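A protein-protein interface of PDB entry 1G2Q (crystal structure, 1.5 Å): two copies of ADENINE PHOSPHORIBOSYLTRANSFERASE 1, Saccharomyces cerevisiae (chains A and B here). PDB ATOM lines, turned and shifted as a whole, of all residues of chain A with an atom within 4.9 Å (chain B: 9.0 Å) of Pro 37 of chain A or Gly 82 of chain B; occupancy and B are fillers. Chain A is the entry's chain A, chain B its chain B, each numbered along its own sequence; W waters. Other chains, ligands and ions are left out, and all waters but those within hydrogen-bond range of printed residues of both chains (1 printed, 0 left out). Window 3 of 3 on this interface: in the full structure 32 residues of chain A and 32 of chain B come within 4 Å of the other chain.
Among the printed residues, pairs that only touch across the chains: Phe 34 of chain A with Gly 84 of chain B, Arg 35 of chain A with Tyr 62 of chain B, Arg 35 of chain A with Gly 84 of chain B, Arg 35 of chain A with Phe 85 of chain B, Pro 37 of chain A with Leu 79 of chain B, Pro 37 of chain A with Gly 82 of chain B, Pro 37 of chain A with Val 83 of chain B, Phe 40 of chain A with Pro 75 of chain B, Phe 40 of chain A with Leu 79 of chain B and Gln 41 of chain A with Leu 79 of chain B.
The backbone carbonyl oxygen of Asp 61 of chain B lies within hydrogen-bond range of the backbone NH of Gly 84 of chain B, 3.3 Å away.
The backbone NH (N) of Ile 63 of chain B sits at hydrogen-bond distance from the backbone carbonyl oxygen (O) of Gly 84 of chain B (2.9 Å).
O of Ala 78 of chain B lies within hydrogen-bond range of N of Val 83 of chain B (2.9 Å).
No position is printed for both chains.
The backbone carbonyl oxygen (O) of Phe 34 of chain A lies within hydrogen-bond range of the backbone NH (N) of Phe 85 of chain B, at 2.8 Å.
Water W1 lies within hydrogen-bond range of O of Phe 34 of chain A and O of Val 83 of chain B.
Among the printed residues, no Asp or Glu carboxylate lies within 4 Å of a Lys or Arg side-chain nitrogen of the other chain.
Printed residues of chain B within 4 Å of Phe 34 of chain A: Gly 84 (3.7 Å) and Phe 85 (2.8 Å).
No residue of chain B comes within 4 Å of Asn 36 of chain A.
Pro 37 of chain A touches just these residues of chain B: Leu 79, Gly 82 and Val 83.
No residue of chain B comes within 4 Å of Gly 38 of chain A.
Of the printed residues of chain B, Phe 40 of chain A touches Pro 75 (3.4 Å) and Leu 79 (3.9 Å).
Ile 63 of chain B touches none of the printed residues of chain A.
Printed residues of chain A within 4 Å of Pro 75 of chain B: Phe 40.
The nearest residue of chain B that does not touch Pro 37 of chain A is Gly 84 of chain B (4.1 Å).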
ATOM      1  N   PHE A  34      22.088  15.467 -19.653  1.00  0.00           N
ATOM      2  CA  PHE A  34      22.873  14.475 -18.924  1.00  0.00           C
ATOM      3  C   PHE A  34      22.181  13.134 -18.731  1.00  0.00           C
ATOM      4  O   PHE A  34      22.834  12.131 -18.433  1.00  0.00           O
ATOM      5  CB  PHE A  34      23.287  15.045 -17.564  1.00  0.00           C
ATOM      6  CG  PHE A  34      24.054  16.325 -17.667  1.00  0.00           C
ATOM      7  CD1 PHE A  34      23.400  17.553 -17.657  1.00  0.00           C
ATOM      8  CD2 PHE A  34      25.434  16.301 -17.839  1.00  0.00           C
ATOM      9  CE1 PHE A  34      24.108  18.744 -17.817  1.00  0.00           C
ATOM     10  CE2 PHE A  34      26.155  17.482 -18.001  1.00  0.00           C
ATOM     11  CZ  PHE A  34      25.491  18.709 -17.991  1.00  0.00           C
ATOM     12  N   ARG A  35      20.863  13.121 -18.903  1.00  0.00           N
ATOM     13  CA  ARG A  35      20.079  11.896 -18.747  1.00  0.00           C
ATOM     14  C   ARG A  35      20.295  10.928 -19.899  1.00  0.00           C
ATOM     15  O   ARG A  35      20.027   9.731 -19.768  1.00  0.00           O
ATOM     16  CB  ARG A  35      18.587  12.222 -18.677  1.00  0.00           C
ATOM     17  CG  ARG A  35      18.176  13.114 -17.534  1.00  0.00           C
ATOM     18  CD  ARG A  35      16.698  13.450 -17.661  1.00  0.00           C
ATOM     19  NE  ARG A  35      16.293  14.494 -16.727  1.00  0.00           N
ATOM     20  CZ  ARG A  35      15.146  15.160 -16.802  1.00  0.00           C
ATOM     21  NH1 ARG A  35      14.278  14.893 -17.775  1.00  0.00           N
ATOM     22  NH2 ARG A  35      14.864  16.093 -15.905  1.00  0.00           N
ATOM     23  N   ASN A  36      20.765  11.454 -21.026  1.00  0.00           N
ATOM     24  CA  ASN A  36      20.997  10.660 -22.231  1.00  0.00           C
ATOM     25  C   ASN A  36      22.483  10.703 -22.581  1.00  0.00           C
ATOM     26  O   ASN A  36      22.996  11.742 -22.988  1.00  0.00           O
ATOM     27  CB  ASN A  36      20.158  11.244 -23.373  1.00  0.00           C
ATOM     28  CG  ASN A  36      20.203  10.403 -24.626  1.00  0.00           C
ATOM     29  OD1 ASN A  36      21.253  10.233 -25.236  1.00  0.00           O
ATOM     30  ND2 ASN A  36      19.049   9.868 -25.019  1.00  0.00           N
ATOM     31  N   PRO A  37      23.194   9.572 -22.428  1.00  0.00           N
ATOM     32  CA  PRO A  37      24.629   9.548 -22.737  1.00  0.00           C
ATOM     33  C   PRO A  37      24.988  10.000 -24.147  1.00  0.00           C
ATOM     34  O   PRO A  37      26.046  10.592 -24.365  1.00  0.00           O
ATOM     35  CB  PRO A  37      25.028   8.098 -22.448  1.00  0.00           C
ATOM     36  CG  PRO A  37      23.760   7.334 -22.670  1.00  0.00           C
ATOM     37  CD  PRO A  37      22.714   8.231 -22.053  1.00  0.00           C
ATOM     38  N   GLY A  38      24.109   9.723 -25.102  1.00  0.00           N
ATOM     39  CA  GLY A  38      24.368  10.144 -26.464  1.00  0.00           C
ATOM     40  C   GLY A  38      24.381  11.660 -26.576  1.00  0.00           C
ATOM     41  O   GLY A  38      25.233  12.233 -27.257  1.00  0.00           O
ATOM     42  N   LEU A  39      23.432  12.315 -25.911  1.00  0.00           N
ATOM     43  CA  LEU A  39      23.349  13.776 -25.931  1.00  0.00           C
ATOM     44  C   LEU A  39      24.484  14.387 -25.116  1.00  0.00           C
ATOM     45  O   LEU A  39      25.110  15.368 -25.531  1.00  0.00           O
ATOM     46  CB  LEU A  39      22.011  14.255 -25.358  1.00  0.00           C
ATOM     47  CG  LEU A  39      20.747  14.078 -26.199  1.00  0.00           C
ATOM     48  CD1 LEU A  39      19.539  14.576 -25.403  1.00  0.00           C
ATOM     49  CD2 LEU A  39      20.886  14.855 -27.502  1.00  0.00           C
ATOM     50  N   PHE A  40      24.739  13.809 -23.947  1.00  0.00           N
ATOM     51  CA  PHE A  40      25.800  14.289 -23.073  1.00  0.00           C
ATOM     52  C   PHE A  40      27.114  14.291 -23.859  1.00  0.00           C
ATOM     53  O   PHE A  40      27.854  15.274 -23.845  1.00  0.00           O
ATOM     54  CB  PHE A  40      25.882  13.381 -21.834  1.00  0.00           C
ATOM     55  CG  PHE A  40      26.812  13.874 -20.745  1.00  0.00           C
ATOM     56  CD1 PHE A  40      27.019  13.097 -19.610  1.00  0.00           C
ATOM     57  CD2 PHE A  40      27.490  15.087 -20.858  1.00  0.00           C
ATOM     58  CE1 PHE A  40      27.888  13.512 -18.601  1.00  0.00           C
ATOM     59  CE2 PHE A  40      28.365  15.516 -19.852  1.00  0.00           C
ATOM     60  CZ  PHE A  40      28.562  14.720 -18.721  1.00  0.00           C
ATOM     61  N   GLN A  41      27.399  13.203 -24.571  1.00  0.00           N
ATOM     62  CA  GLN A  41      28.636  13.152 -25.339  1.00  0.00           C
ATOM     63  C   GLN A  41      28.678  14.238 -26.417  1.00  0.00           C
ATOM     64  O   GLN A  41      29.745  14.780 -26.711  1.00  0.00           O
ATOM     65  CB  GLN A  41      28.832  11.764 -25.960  1.00  0.00           C
ATOM     66  CG  GLN A  41      30.133  11.630 -26.740  1.00  0.00           C
ATOM     67  CD  GLN A  41      31.361  11.931 -25.895  1.00  0.00           C
ATOM     68  OE1 GLN A  41      32.304  12.571 -26.361  1.00  0.00           O
ATOM     69  NE2 GLN A  41      31.358  11.465 -24.651  1.00  0.00           N
ATOM     70  N   LYS B  48      34.124   2.007 -12.444  1.00  0.00           N
ATOM     71  CA  LYS B  48      33.581   1.277 -13.584  1.00  0.00           C
ATOM     72  C   LYS B  48      33.839  -0.216 -13.397  1.00  0.00           C
ATOM     73  O   LYS B  48      32.928  -1.028 -13.535  1.00  0.00           O
ATOM     74  CB  LYS B  48      34.224   1.767 -14.884  1.00  0.00           C
ATOM     75  CG  LYS B  48      33.702   1.089 -16.143  1.00  0.00           C
ATOM     76  CD  LYS B  48      34.280   1.744 -17.391  1.00  0.00           C
ATOM     77  CE  LYS B  48      33.764   1.097 -18.674  1.00  0.00           C
ATOM     78  NZ  LYS B  48      34.227  -0.313 -18.824  1.00  0.00           N
ATOM     79  N   GLU B  52      31.092  -3.205 -12.890  1.00  0.00           N
ATOM     80  CA  GLU B  52      31.028  -4.282 -13.871  1.00  0.00           C
ATOM     81  C   GLU B  52      31.122  -5.632 -13.174  1.00  0.00           C
ATOM     82  O   GLU B  52      30.580  -6.629 -13.655  1.00  0.00           O
ATOM     83  CB  GLU B  52      32.164  -4.153 -14.887  1.00  0.00           C
ATOM     84  CG  GLU B  52      32.132  -2.866 -15.690  1.00  0.00           C
ATOM     85  CD  GLU B  52      33.262  -2.777 -16.692  1.00  0.00           C
ATOM     86  OE1 GLU B  52      34.404  -3.137 -16.337  1.00  0.00           O
ATOM     87  OE2 GLU B  52      33.007  -2.336 -17.832  1.00  0.00           O
ATOM     88  N   LYS B  59      21.224  -4.617 -15.246  1.00  0.00           N
ATOM     89  CA  LYS B  59      21.368  -3.384 -16.005  1.00  0.00           C
ATOM     90  C   LYS B  59      21.278  -2.144 -15.129  1.00  0.00           C
ATOM     91  O   LYS B  59      20.341  -1.996 -14.346  1.00  0.00           O
ATOM     92  CB  LYS B  59      20.297  -3.307 -17.099  1.00  0.00           C
ATOM     93  CG  LYS B  59      20.382  -2.051 -17.953  1.00  0.00           C
ATOM     94  CD  LYS B  59      19.279  -2.001 -19.001  1.00  0.00           C
ATOM     95  CE  LYS B  59      19.360  -0.726 -19.827  1.00  0.00           C
ATOM     96  NZ  LYS B  59      18.280  -0.649 -20.853  1.00  0.00           N
ATOM     97  N   ILE B  60      22.266  -1.262 -15.255  1.00  0.00           N
ATOM     98  CA  ILE B  60      22.271  -0.008 -14.508  1.00  0.00           C
ATOM     99  C   ILE B  60      21.721   1.037 -15.471  1.00  0.00           C
ATOM    100  O   ILE B  60      22.183   1.147 -16.609  1.00  0.00           O
ATOM    101  CB  ILE B  60      23.698   0.404 -14.077  1.00  0.00           C
ATOM    102  CG1 ILE B  60      24.249  -0.600 -13.061  1.00  0.00           C
ATOM    103  CG2 ILE B  60      23.673   1.815 -13.484  1.00  0.00           C
ATOM    104  CD1 ILE B  60      25.700  -0.355 -12.672  1.00  0.00           C
ATOM    105  N   ASP B  61      20.729   1.800 -15.019  1.00  0.00           N
ATOM    106  CA  ASP B  61      20.113   2.815 -15.861  1.00  0.00           C
ATOM    107  C   ASP B  61      20.651   4.225 -15.636  1.00  0.00           C
ATOM    108  O   ASP B  61      20.816   4.993 -16.591  1.00  0.00           O
ATOM    109  CB  ASP B  61      18.593   2.801 -15.654  1.00  0.00           C
ATOM    110  CG  ASP B  61      17.955   1.497 -16.110  1.00  0.00           C
ATOM    111  OD1 ASP B  61      18.011   1.207 -17.327  1.00  0.00           O
ATOM    112  OD2 ASP B  61      17.402   0.775 -15.254  1.00  0.00           O
ATOM    113  N   TYR B  62      20.915   4.565 -14.377  1.00  0.00           N
ATOM    114  CA  TYR B  62      21.418   5.895 -14.053  1.00  0.00           C
ATOM    115  C   TYR B  62      22.381   5.936 -12.886  1.00  0.00           C
ATOM    116  O   TYR B  62      22.368   5.082 -11.996  1.00  0.00           O
ATOM    117  CB  TYR B  62      20.277   6.854 -13.679  1.00  0.00           C
ATOM    118  CG  TYR B  62      19.221   7.035 -14.734  1.00  0.00           C
ATOM    119  CD1 TYR B  62      18.152   6.149 -14.831  1.00  0.00           C
ATOM    120  CD2 TYR B  62      19.326   8.055 -15.679  1.00  0.00           C
ATOM    121  CE1 TYR B  62      17.214   6.269 -15.849  1.00  0.00           C
ATOM    122  CE2 TYR B  62      18.395   8.184 -16.703  1.00  0.00           C
ATOM    123  CZ  TYR B  62      17.343   7.283 -16.782  1.00  0.00           C
ATOM    124  OH  TYR B  62      16.442   7.388 -17.818  1.00  0.00           O
ATOM    125  N   ILE B  63      23.211   6.969 -12.914  1.00  0.00           N
ATOM    126  CA  ILE B  63      24.124   7.267 -11.836  1.00  0.00           C
ATOM    127  C   ILE B  63      23.450   8.504 -11.246  1.00  0.00           C
ATOM    128  O   ILE B  63      23.126   9.447 -11.978  1.00  0.00           O
ATOM    129  CB  ILE B  63      25.529   7.675 -12.334  1.00  0.00           C
ATOM    130  CG1 ILE B  63      26.249   6.470 -12.942  1.00  0.00           C
ATOM    131  CG2 ILE B  63      26.340   8.267 -11.177  1.00  0.00           C
ATOM    132  CD1 ILE B  63      26.454   5.308 -11.977  1.00  0.00           C
ATOM    133  N   GLY B  74      30.554  11.745 -10.792  1.00  0.00           N
ATOM    134  CA  GLY B  74      29.366  11.012 -11.200  1.00  0.00           C
ATOM    135  C   GLY B  74      29.005  11.096 -12.675  1.00  0.00           C
ATOM    136  O   GLY B  74      28.754  10.069 -13.314  1.00  0.00           O
ATOM    137  N   PRO B  75      28.955  12.302 -13.249  1.00  0.00           N
ATOM    138  CA  PRO B  75      28.608  12.429 -14.667  1.00  0.00           C
ATOM    139  C   PRO B  75      29.589  11.699 -15.587  1.00  0.00           C
ATOM    140  O   PRO B  75      29.178  11.072 -16.562  1.00  0.00           O
ATOM    141  CB  PRO B  75      28.615  13.942 -14.890  1.00  0.00           C
ATOM    142  CG  PRO B  75      28.233  14.486 -13.530  1.00  0.00           C
ATOM    143  CD  PRO B  75      29.052  13.625 -12.609  1.00  0.00           C
ATOM    144  N   THR B  76      30.880  11.789 -15.279  1.00  0.00           N
ATOM    145  CA  THR B  76      31.894  11.133 -16.097  1.00  0.00           C
ATOM    146  C   THR B  76      31.769   9.615 -15.969  1.00  0.00           C
ATOM    147  O   THR B  76      31.923   8.889 -16.950  1.00  0.00           O
ATOM    148  CB  THR B  76      33.309  11.588 -15.693  1.00  0.00           C
ATOM    149  OG1 THR B  76      33.420  13.010 -15.868  1.00  0.00           O
ATOM    150  CG2 THR B  76      34.354  10.902 -16.557  1.00  0.00           C
ATOM    151  N   LEU B  77      31.472   9.135 -14.765  1.00  0.00           N
ATOM    152  CA  LEU B  77      31.307   7.697 -14.572  1.00  0.00           C
ATOM    153  C   LEU B  77      30.112   7.231 -15.402  1.00  0.00           C
ATOM    154  O   LEU B  77      30.151   6.175 -16.028  1.00  0.00           O
ATOM    155  CB  LEU B  77      31.074   7.381 -13.092  1.00  0.00           C
ATOM    156  CG  LEU B  77      30.724   5.941 -12.690  1.00  0.00           C
ATOM    157  CD1 LEU B  77      31.834   4.981 -13.107  1.00  0.00           C
ATOM    158  CD2 LEU B  77      30.512   5.893 -11.187  1.00  0.00           C
ATOM    159  N   ALA B  78      29.047   8.025 -15.403  1.00  0.00           N
ATOM    160  CA  ALA B  78      27.849   7.679 -16.161  1.00  0.00           C
ATOM    161  C   ALA B  78      28.180   7.523 -17.640  1.00  0.00           C
ATOM    162  O   ALA B  78      27.807   6.535 -18.269  1.00  0.00           O
ATOM    163  CB  ALA B  78      26.780   8.759 -15.970  1.00  0.00           C
ATOM    164  N   LEU B  79      28.893   8.500 -18.186  1.00  0.00           N
ATOM    165  CA  LEU B  79      29.266   8.473 -19.592  1.00  0.00           C
ATOM    166  C   LEU B  79      30.178   7.281 -19.880  1.00  0.00           C
ATOM    167  O   LEU B  79      30.043   6.619 -20.916  1.00  0.00           O
ATOM    168  CB  LEU B  79      29.949   9.796 -19.961  1.00  0.00           C
ATOM    169  CG  LEU B  79      29.845  10.322 -21.392  1.00  0.00           C
ATOM    170  CD1 LEU B  79      28.421  10.168 -21.919  1.00  0.00           C
ATOM    171  CD2 LEU B  79      30.268  11.785 -21.405  1.00  0.00           C
ATOM    172  N   ALA B  80      31.099   6.994 -18.961  1.00  0.00           N
ATOM    173  CA  ALA B  80      32.023   5.873 -19.128  1.00  0.00           C
ATOM    174  C   ALA B  80      31.264   4.550 -19.180  1.00  0.00           C
ATOM    175  O   ALA B  80      31.679   3.612 -19.862  1.00  0.00           O
ATOM    176  CB  ALA B  80      33.038   5.853 -17.980  1.00  0.00           C
ATOM    177  N   LEU B  81      30.156   4.482 -18.451  1.00  0.00           N
ATOM    178  CA  LEU B  81      29.327   3.282 -18.403  1.00  0.00           C
ATOM    179  C   LEU B  81      28.282   3.258 -19.512  1.00  0.00           C
ATOM    180  O   LEU B  81      27.684   2.217 -19.783  1.00  0.00           O
ATOM    181  CB  LEU B  81      28.602   3.190 -17.060  1.00  0.00           C
ATOM    182  CG  LEU B  81      29.427   2.916 -15.806  1.00  0.00           C
ATOM    183  CD1 LEU B  81      28.553   3.106 -14.576  1.00  0.00           C
ATOM    184  CD2 LEU B  81      29.999   1.505 -15.863  1.00  0.00           C
ATOM    185  N   GLY B  82      28.056   4.403 -20.143  1.00  0.00           N
ATOM    186  CA  GLY B  82      27.066   4.478 -21.202  1.00  0.00           C
ATOM    187  C   GLY B  82      25.665   4.595 -20.640  1.00  0.00           C
ATOM    188  O   GLY B  82      24.703   4.128 -21.253  1.00  0.00           O
ATOM    189  N   VAL B  83      25.546   5.213 -19.465  1.00  0.00           N
ATOM    190  CA  VAL B  83      24.247   5.385 -18.818  1.00  0.00           C
ATOM    191  C   VAL B  83      23.969   6.859 -18.533  1.00  0.00           C
ATOM    192  O   VAL B  83      24.836   7.708 -18.725  1.00  0.00           O
ATOM    193  CB  VAL B  83      24.162   4.578 -17.494  1.00  0.00           C
ATOM    194  CG1 VAL B  83      24.528   3.119 -17.755  1.00  0.00           C
ATOM    195  CG2 VAL B  83      25.085   5.183 -16.432  1.00  0.00           C
ATOM    196  N   GLY B  84      22.759   7.161 -18.074  1.00  0.00           N
ATOM    197  CA  GLY B  84      22.416   8.544 -17.794  1.00  0.00           C
ATOM    198  C   GLY B  84      22.857   9.026 -16.428  1.00  0.00           C
ATOM    199  O   GLY B  84      23.172   8.223 -15.544  1.00  0.00           O
ATOM    200  N   PHE B  85      22.894  10.345 -16.259  1.00  0.00           N
ATOM    201  CA  PHE B  85      23.258  10.948 -14.979  1.00  0.00           C
ATOM    202  C   PHE B  85      22.141  11.881 -14.524  1.00  0.00           C
ATOM    203  O   PHE B  85      21.619  12.661 -15.314  1.00  0.00           O
ATOM    204  CB  PHE B  85      24.539  11.778 -15.079  1.00  0.00           C
ATOM    205  CG  PHE B  85      24.864  12.505 -13.802  1.00  0.00           C
ATOM    206  CD1 PHE B  85      25.542  11.857 -12.776  1.00  0.00           C
ATOM    207  CD2 PHE B  85      24.410  13.809 -13.591  1.00  0.00           C
ATOM    208  CE1 PHE B  85      25.763  12.484 -11.551  1.00  0.00           C
ATOM    209  CE2 PHE B  85      24.625  14.450 -12.367  1.00  0.00           C
ATOM    210  CZ  PHE B  85      25.300  13.791 -11.346  1.00  0.00           C
HETATM  211  O   HOH W   1      24.904  10.486 -19.625  1.00  0.00           O
